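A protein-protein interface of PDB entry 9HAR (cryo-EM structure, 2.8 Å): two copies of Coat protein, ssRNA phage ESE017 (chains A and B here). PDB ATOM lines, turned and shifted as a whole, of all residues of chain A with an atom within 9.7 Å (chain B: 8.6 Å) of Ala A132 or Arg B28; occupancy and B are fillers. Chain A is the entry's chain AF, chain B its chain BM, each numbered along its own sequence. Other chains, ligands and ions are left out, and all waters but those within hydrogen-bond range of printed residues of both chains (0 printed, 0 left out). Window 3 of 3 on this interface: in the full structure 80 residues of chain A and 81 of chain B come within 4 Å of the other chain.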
ATOM      1  N   ALA A   1       0.766  14.466   7.426  1.00  0.00           N
ATOM      2  CA  ALA A   1      -0.240  13.494   7.018  1.00  0.00           C
ATOM      3  C   ALA A   1      -0.447  13.527   5.507  1.00  0.00           C
ATOM      4  O   ALA A   1       0.349  14.114   4.783  1.00  0.00           O
ATOM      5  CB  ALA A   1      -1.545  13.749   7.739  1.00  0.00           C
ATOM      6  N   ILE A   2      -1.527  12.891   5.044  1.00  0.00           N
ATOM      7  CA  ILE A   2      -1.784  12.791   3.609  1.00  0.00           C
ATOM      8  C   ILE A   2      -2.003  14.169   3.003  1.00  0.00           C
ATOM      9  O   ILE A   2      -1.454  14.491   1.942  1.00  0.00           O
ATOM     10  CB  ILE A   2      -2.983  11.861   3.346  1.00  0.00           C
ATOM     11  CG1 ILE A   2      -2.589  10.403   3.562  1.00  0.00           C
ATOM     12  CG2 ILE A   2      -3.523  12.065   1.943  1.00  0.00           C
ATOM     13  CD1 ILE A   2      -3.770   9.470   3.628  1.00  0.00           C
ATOM     14  N   ALA A   3      -2.805  15.003   3.658  1.00  0.00           N
ATOM     15  CA  ALA A   3      -3.061  16.347   3.160  1.00  0.00           C
ATOM     16  C   ALA A   3      -1.797  17.192   3.237  1.00  0.00           C
ATOM     17  O   ALA A   3      -1.135  17.246   4.276  1.00  0.00           O
ATOM     18  CB  ALA A   3      -4.184  17.004   3.959  1.00  0.00           C
ATOM     19  N   ASN A   4      -1.465  17.849   2.122  1.00  0.00           N
ATOM     20  CA  ASN A   4      -0.293  18.722   2.020  1.00  0.00           C
ATOM     21  C   ASN A   4       1.005  17.958   2.267  1.00  0.00           C
ATOM     22  O   ASN A   4       1.999  18.520   2.729  1.00  0.00           O
ATOM     23  CB  ASN A   4      -0.407  19.920   2.965  1.00  0.00           C
ATOM     24  CG  ASN A   4      -1.206  21.057   2.364  1.00  0.00           C
ATOM     25  OD1 ASN A   4      -0.936  21.499   1.247  1.00  0.00           O
ATOM     26  ND2 ASN A   4      -2.203  21.534   3.101  1.00  0.00           N
ATOM     27  N   ASP A 121       4.883  11.224   6.305  1.00  0.00           N
ATOM     28  CA  ASP A 121       3.509  11.714   6.261  1.00  0.00           C
ATOM     29  C   ASP A 121       2.507  10.570   6.232  1.00  0.00           C
ATOM     30  O   ASP A 121       1.413  10.682   6.794  1.00  0.00           O
ATOM     31  CB  ASP A 121       3.309  12.618   5.045  1.00  0.00           C
ATOM     32  CG  ASP A 121       4.410  13.639   4.893  1.00  0.00           C
ATOM     33  OD1 ASP A 121       4.724  14.325   5.888  1.00  0.00           O
ATOM     34  OD2 ASP A 121       4.946  13.773   3.774  1.00  0.00           O
ATOM     35  N   TYR A 122       2.858   9.467   5.582  1.00  0.00           N
ATOM     36  CA  TYR A 122       1.938   8.358   5.383  1.00  0.00           C
ATOM     37  C   TYR A 122       2.076   7.270   6.439  1.00  0.00           C
ATOM     38  O   TYR A 122       1.390   6.248   6.341  1.00  0.00           O
ATOM     39  CB  TYR A 122       2.138   7.774   3.984  1.00  0.00           C
ATOM     40  CG  TYR A 122       2.215   8.851   2.928  1.00  0.00           C
ATOM     41  CD1 TYR A 122       1.071   9.503   2.492  1.00  0.00           C
ATOM     42  CD2 TYR A 122       3.433   9.236   2.389  1.00  0.00           C
ATOM     43  CE1 TYR A 122       1.133  10.493   1.539  1.00  0.00           C
ATOM     44  CE2 TYR A 122       3.507  10.231   1.435  1.00  0.00           C
ATOM     45  CZ  TYR A 122       2.353  10.854   1.015  1.00  0.00           C
ATOM     46  OH  TYR A 122       2.418  11.842   0.063  1.00  0.00           O
ATOM     47  N   ASP A 124       0.990   7.202   9.544  1.00  0.00           N
ATOM     48  CA  ASP A 124      -0.292   6.985  10.204  1.00  0.00           C
ATOM     49  C   ASP A 124      -1.294   6.325   9.265  1.00  0.00           C
ATOM     50  O   ASP A 124      -2.121   5.515   9.695  1.00  0.00           O
ATOM     51  CB  ASP A 124      -0.842   8.310  10.735  1.00  0.00           C
ATOM     52  CG  ASP A 124       0.172   9.069  11.574  1.00  0.00           C
ATOM     53  OD1 ASP A 124      -0.234   9.998  12.303  1.00  0.00           O
ATOM     54  OD2 ASP A 124       1.374   8.735  11.505  1.00  0.00           O
ATOM     55  N   PHE A 125      -1.244   6.664   7.977  1.00  0.00           N
ATOM     56  CA  PHE A 125      -2.137   6.026   7.018  1.00  0.00           C
ATOM     57  C   PHE A 125      -1.868   4.529   6.921  1.00  0.00           C
ATOM     58  O   PHE A 125      -2.797   3.714   6.928  1.00  0.00           O
ATOM     59  CB  PHE A 125      -2.001   6.674   5.642  1.00  0.00           C
ATOM     60  CG  PHE A 125      -2.764   5.952   4.578  1.00  0.00           C
ATOM     61  CD1 PHE A 125      -4.142   5.894   4.616  1.00  0.00           C
ATOM     62  CD2 PHE A 125      -2.099   5.297   3.559  1.00  0.00           C
ATOM     63  CE1 PHE A 125      -4.842   5.218   3.648  1.00  0.00           C
ATOM     64  CE2 PHE A 125      -2.795   4.619   2.596  1.00  0.00           C
ATOM     65  CZ  PHE A 125      -4.167   4.579   2.636  1.00  0.00           C
ATOM     66  N   ALA A 128      -2.265   3.148  11.303  1.00  0.00           N
ATOM     67  CA  ALA A 128      -3.547   3.273  11.980  1.00  0.00           C
ATOM     68  C   ALA A 128      -4.710   3.533  11.033  1.00  0.00           C
ATOM     69  O   ALA A 128      -5.833   3.730  11.506  1.00  0.00           O
ATOM     70  CB  ALA A 128      -3.482   4.390  13.025  1.00  0.00           C
ATOM     71  N   GLN A 129      -4.474   3.540   9.720  1.00  0.00           N
ATOM     72  CA  GLN A 129      -5.510   3.807   8.717  1.00  0.00           C
ATOM     73  C   GLN A 129      -6.081   5.218   8.856  1.00  0.00           C
ATOM     74  O   GLN A 129      -7.257   5.467   8.592  1.00  0.00           O
ATOM     75  CB  GLN A 129      -6.624   2.760   8.778  1.00  0.00           C
ATOM     76  CG  GLN A 129      -6.130   1.340   8.813  1.00  0.00           C
ATOM     77  CD  GLN A 129      -6.694   0.522   7.686  1.00  0.00           C
ATOM     78  OE1 GLN A 129      -5.980   0.131   6.762  1.00  0.00           O
ATOM     79  NE2 GLN A 129      -7.982   0.236   7.762  1.00  0.00           N
ATOM     80  N   ALA A 130      -5.224   6.155   9.262  1.00  0.00           N
ATOM     81  CA  ALA A 130      -5.624   7.551   9.425  1.00  0.00           C
ATOM     82  C   ALA A 130      -5.665   8.215   8.052  1.00  0.00           C
ATOM     83  O   ALA A 130      -4.704   8.836   7.593  1.00  0.00           O
ATOM     84  CB  ALA A 130      -4.675   8.272  10.372  1.00  0.00           C
ATOM     85  N   LEU A 131      -6.812   8.072   7.386  1.00  0.00           N
ATOM     86  CA  LEU A 131      -7.035   8.716   6.097  1.00  0.00           C
ATOM     87  C   LEU A 131      -6.958  10.228   6.248  1.00  0.00           C
ATOM     88  O   LEU A 131      -6.093  10.879   5.654  1.00  0.00           O
ATOM     89  CB  LEU A 131      -8.393   8.323   5.516  1.00  0.00           C
ATOM     90  CG  LEU A 131      -8.350   7.309   4.378  1.00  0.00           C
ATOM     91  CD1 LEU A 131      -9.735   7.101   3.795  1.00  0.00           C
ATOM     92  CD2 LEU A 131      -7.366   7.749   3.321  1.00  0.00           C
ATOM     93  N   ALA A 132      -7.858  10.790   7.042  1.00  0.00           N
ATOM     94  CA  ALA A 132      -7.808  12.205   7.364  1.00  0.00           C
ATOM     95  C   ALA A 132      -6.967  12.401   8.615  1.00  0.00           C
ATOM     96  O   ALA A 132      -7.363  11.979   9.698  1.00  0.00           O
ATOM     97  CB  ALA A 132      -9.209  12.763   7.561  1.00  0.00           C
ATOM     98  OXT ALA A 132      -5.878  12.972   8.580  1.00  0.00           O
ATOM     99  N   GLU B  25      -5.380  17.335  -1.721  1.00  0.00           N
ATOM    100  CA  GLU B  25      -6.547  16.473  -1.792  1.00  0.00           C
ATOM    101  C   GLU B  25      -7.634  17.105  -2.653  1.00  0.00           C
ATOM    102  O   GLU B  25      -7.752  18.328  -2.753  1.00  0.00           O
ATOM    103  CB  GLU B  25      -7.076  16.165  -0.393  1.00  0.00           C
ATOM    104  CG  GLU B  25      -7.806  17.296   0.275  1.00  0.00           C
ATOM    105  CD  GLU B  25      -8.822  16.808   1.281  1.00  0.00           C
ATOM    106  OE1 GLU B  25      -9.284  15.656   1.151  1.00  0.00           O
ATOM    107  OE2 GLU B  25      -9.152  17.577   2.207  1.00  0.00           O
ATOM    108  N   LEU B  26      -8.425  16.248  -3.295  1.00  0.00           N
ATOM    109  CA  LEU B  26      -9.491  16.708  -4.180  1.00  0.00           C
ATOM    110  C   LEU B  26     -10.856  16.416  -3.574  1.00  0.00           C
ATOM    111  O   LEU B  26     -11.622  17.348  -3.331  1.00  0.00           O
ATOM    112  CB  LEU B  26      -9.344  16.049  -5.551  1.00  0.00           C
ATOM    113  CG  LEU B  26      -8.122  16.403  -6.395  1.00  0.00           C
ATOM    114  CD1 LEU B  26      -7.968  15.414  -7.531  1.00  0.00           C
ATOM    115  CD2 LEU B  26      -8.256  17.810  -6.937  1.00  0.00           C
ATOM    116  N   VAL B  27     -11.179  15.152  -3.304  1.00  0.00           N
ATOM    117  CA  VAL B  27     -12.466  14.757  -2.755  1.00  0.00           C
ATOM    118  C   VAL B  27     -12.218  13.721  -1.667  1.00  0.00           C
ATOM    119  O   VAL B  27     -11.079  13.391  -1.341  1.00  0.00           O
ATOM    120  CB  VAL B  27     -13.417  14.200  -3.831  1.00  0.00           C
ATOM    121  CG1 VAL B  27     -13.872  15.307  -4.752  1.00  0.00           C
ATOM    122  CG2 VAL B  27     -12.742  13.098  -4.613  1.00  0.00           C
ATOM    123  N   ARG B  28     -13.302  13.217  -1.094  1.00  0.00           N
ATOM    124  CA  ARG B  28     -13.203  12.206  -0.050  1.00  0.00           C
ATOM    125  C   ARG B  28     -14.050  10.972  -0.299  1.00  0.00           C
ATOM    126  O   ARG B  28     -13.630   9.870   0.060  1.00  0.00           O
ATOM    127  CB  ARG B  28     -13.571  12.807   1.309  1.00  0.00           C
ATOM    128  CG  ARG B  28     -12.411  13.514   1.969  1.00  0.00           C
ATOM    129  CD  ARG B  28     -12.793  14.038   3.330  1.00  0.00           C
ATOM    130  NE  ARG B  28     -11.791  14.964   3.838  1.00  0.00           N
ATOM    131  CZ  ARG B  28     -10.595  14.610   4.283  1.00  0.00           C
ATOM    132  NH1 ARG B  28     -10.221  13.342   4.329  1.00  0.00           N
ATOM    133  NH2 ARG B  28      -9.754  15.551   4.702  1.00  0.00           N
ATOM    134  N   ASN B  29     -15.210  11.123  -0.946  1.00  0.00           N
ATOM    135  CA  ASN B  29     -16.275  10.120  -1.023  1.00  0.00           C
ATOM    136  C   ASN B  29     -16.252   9.094   0.111  1.00  0.00           C
ATOM    137  O   ASN B  29     -16.032   9.445   1.274  1.00  0.00           O
ATOM    138  CB  ASN B  29     -16.319   9.399  -2.389  1.00  0.00           C
ATOM    139  CG  ASN B  29     -14.949   9.070  -2.980  1.00  0.00           C
ATOM    140  OD1 ASN B  29     -13.928   9.641  -2.621  1.00  0.00           O
ATOM    141  ND2 ASN B  29     -14.939   8.127  -3.914  1.00  0.00           N
ATOM    142  N   ASN B  30     -16.512   7.832  -0.213  1.00  0.00           N
ATOM    143  CA  ASN B  30     -16.802   6.812   0.794  1.00  0.00           C
ATOM    144  C   ASN B  30     -15.502   6.208   1.313  1.00  0.00           C
ATOM    145  O   ASN B  30     -14.913   5.333   0.672  1.00  0.00           O
ATOM    146  CB  ASN B  30     -17.704   5.734   0.205  1.00  0.00           C
ATOM    147  CG  ASN B  30     -19.165   5.981   0.495  1.00  0.00           C
ATOM    148  OD1 ASN B  30     -19.592   7.123   0.648  1.00  0.00           O
ATOM    149  ND2 ASN B  30     -19.944   4.908   0.567  1.00  0.00           N
ATOM    150  N   SER B  31     -15.063   6.668   2.484  1.00  0.00           N
ATOM    151  CA  SER B  31     -13.905   6.109   3.183  1.00  0.00           C
ATOM    152  C   SER B  31     -12.678   6.067   2.277  1.00  0.00           C
ATOM    153  O   SER B  31     -11.898   5.114   2.273  1.00  0.00           O
ATOM    154  CB  SER B  31     -14.223   4.723   3.739  1.00  0.00           C
ATOM    155  OG  SER B  31     -14.088   3.730   2.741  1.00  0.00           O
ATOM    156  N   GLU B  32     -12.519   7.129   1.495  1.00  0.00           N
ATOM    157  CA  GLU B  32     -11.461   7.228   0.503  1.00  0.00           C
ATOM    158  C   GLU B  32     -10.849   8.618   0.621  1.00  0.00           C
ATOM    159  O   GLU B  32     -11.318   9.461   1.389  1.00  0.00           O
ATOM    160  CB  GLU B  32     -12.020   6.940  -0.897  1.00  0.00           C
ATOM    161  CG  GLU B  32     -10.976   6.629  -1.953  1.00  0.00           C
ATOM    162  CD  GLU B  32     -11.392   7.092  -3.332  1.00  0.00           C
ATOM    163  OE1 GLU B  32     -10.504   7.452  -4.131  1.00  0.00           O
ATOM    164  OE2 GLU B  32     -12.608   7.094  -3.615  1.00  0.00           O
ATOM    165  N   LEU B  33      -9.776   8.855  -0.125  1.00  0.00           N
ATOM    166  CA  LEU B  33      -9.188  10.184  -0.195  1.00  0.00           C
ATOM    167  C   LEU B  33      -8.491  10.360  -1.533  1.00  0.00           C
ATOM    168  O   LEU B  33      -7.355   9.915  -1.715  1.00  0.00           O
ATOM    169  CB  LEU B  33      -8.211  10.406   0.958  1.00  0.00           C
ATOM    170  CG  LEU B  33      -7.940  11.853   1.365  1.00  0.00           C
ATOM    171  CD1 LEU B  33      -7.572  11.927   2.835  1.00  0.00           C
ATOM    172  CD2 LEU B  33      -6.845  12.468   0.510  1.00  0.00           C
ATOM    173  N   ASN B  34      -9.162  11.013  -2.473  1.00  0.00           N
ATOM    174  CA  ASN B  34      -8.594  11.220  -3.797  1.00  0.00           C
ATOM    175  C   ASN B  34      -7.833  12.536  -3.812  1.00  0.00           C
ATOM    176  O   ASN B  34      -8.419  13.602  -3.614  1.00  0.00           O
ATOM    177  CB  ASN B  34      -9.698  11.210  -4.846  1.00  0.00           C
ATOM    178  CG  ASN B  34      -9.284  10.501  -6.108  1.00  0.00           C
ATOM    179  OD1 ASN B  34      -8.257  10.824  -6.704  1.00  0.00           O
ATOM    180  ND2 ASN B  34     -10.082   9.527  -6.528  1.00  0.00           N
ATOM    181  N   ALA B  35      -6.530  12.463  -4.036  1.00  0.00           N
ATOM    182  CA  ALA B  35      -5.669  13.628  -4.099  1.00  0.00           C
ATOM    183  C   ALA B  35      -5.007  13.701  -5.472  1.00  0.00           C
ATOM    184  O   ALA B  35      -5.310  12.916  -6.375  1.00  0.00           O
ATOM    185  CB  ALA B  35      -4.638  13.579  -2.973  1.00  0.00           C
ATOM    186  N   PHE B  51      -6.178   7.255  -1.946  1.00  0.00           N
ATOM    187  CA  PHE B  51      -5.952   6.519  -0.711  1.00  0.00           C
ATOM    188  C   PHE B  51      -7.268   5.922  -0.232  1.00  0.00           C
ATOM    189  O   PHE B  51      -8.326   6.539  -0.368  1.00  0.00           O
ATOM    190  CB  PHE B  51      -5.392   7.432   0.387  1.00  0.00           C
ATOM    191  CG  PHE B  51      -4.081   8.080   0.047  1.00  0.00           C
ATOM    192  CD1 PHE B  51      -4.042   9.224  -0.730  1.00  0.00           C
ATOM    193  CD2 PHE B  51      -2.894   7.572   0.538  1.00  0.00           C
ATOM    194  CE1 PHE B  51      -2.846   9.829  -1.029  1.00  0.00           C
ATOM    195  CE2 PHE B  51      -1.692   8.176   0.240  1.00  0.00           C
ATOM    196  CZ  PHE B  51      -1.667   9.305  -0.544  1.00  0.00           C
ATOM    197  N   SER B  52      -7.209   4.724   0.345  1.00  0.00           N
ATOM    198  CA  SER B  52      -8.427   4.091   0.839  1.00  0.00           C
ATOM    199  C   SER B  52      -8.113   3.183   2.021  1.00  0.00           C
ATOM    200  O   SER B  52      -7.034   2.591   2.085  1.00  0.00           O
ATOM    201  CB  SER B  52      -9.124   3.293  -0.265  1.00  0.00           C
ATOM    202  OG  SER B  52      -8.187   2.800  -1.202  1.00  0.00           O
ATOM    203  N   VAL B  53      -9.072   3.068   2.942  1.00  0.00           N
ATOM    204  CA  VAL B  53      -8.915   2.244   4.130  1.00  0.00           C
ATOM    205  C   VAL B  53     -10.056   1.238   4.209  1.00  0.00           C
ATOM    206  O   VAL B  53     -11.182   1.483   3.769  1.00  0.00           O
ATOM    207  CB  VAL B  53      -8.841   3.085   5.424  1.00  0.00           C
ATOM    208  CG1 VAL B  53      -7.579   3.921   5.441  1.00  0.00           C
ATOM    209  CG2 VAL B  53     -10.075   3.951   5.562  1.00  0.00           C
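OE2 of Glu B32 lies within hydrogen-bond range of ND2 of Asn B29, at 2.6 Å. The backbone carbonyl oxygen of Phe B51 is in hydrogen-bond range of the backbone NH of Leu B33. OE1 of Glu B32 sits at hydrogen-bond distance from ND2 of Asn B34 (3.2 Å). N of Gln A129 sits at hydrogen-bond distance from O of Asp A124, at 3.1 Å. The side-chain carboxylate (OE2) of Glu B25 lies within salt-bridge range of the guanidinium group (NH2) of Arg B28, at 3.3 Å.
CD2 of Leu B33 touches CG2 of Ile A2, at 3.6 Å. Ile A2 touches Phe B51 (CD1 to CD2, 3.7 Å). CE1 of Tyr A122 touches CZ of Phe B51, 3.7 Å away. Phe A125 touches Phe B51. Val B53 touches Phe A125 (CG1 to CE1, 3.5 Å). CG1 of Val B53 touches O of Gln A129, at 3.5 Å. Leu A131 touches Ser B31 (CD1 to O, 3.3 Å). Leu A131 touches Leu B33 (O to CD1, 3.4 Å). Phe B51 touches Leu A131 (CB to CD2, 3.6 Å). Leu A131 touches Val B53.
Ala A3 touches none of the printed residues of chain B. Ala A132 touches just one residue of chain B: Arg B28 (3.4 Å). Arg B28 touches just one residue of chain A: Ala A132 (3.4 Å). No residue of chain A comes within 4 Å of Asn B29. Printed residues of chain A within 4 Å of Glu B32: Leu A131. Printed residues of chain A within 4 Å of Leu B33: Ile A2 (3.6 Å) and Leu A131 (3.4 Å). Of the printed residues of chain A, Phe B51 touches Ile A2, Tyr A122, Phe A125 and Leu A131. Printed residues of chain A within 4 Å of Ser B52: Phe A125. The nearest residue of chain A that does not touch Arg B28 is Leu A131 (4.9 Å). The nearest printed residue of chain A that does not touch Ser B52 is Leu A131 (4.2 Å).
Hydrophobic or aromatic side chains of chain A within 4 Å of the printed part of chain B: Ile A2, Tyr A122, Phe A125, Leu A131 and Ala A132. Of the 14 printed residues of chain B, 7 touch a printed residue of chain A. Hydrophobic or aromatic side chains of chain B that line the printed part of chain A: Leu B33, Phe B51 and Val B53. Among the printed residues, 13 pairs touch across the chains.
No position is printed for both chains. Of the 13 pairs that touch across the chains among the printed residues, none has its exchanged pair printed and touching as well.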
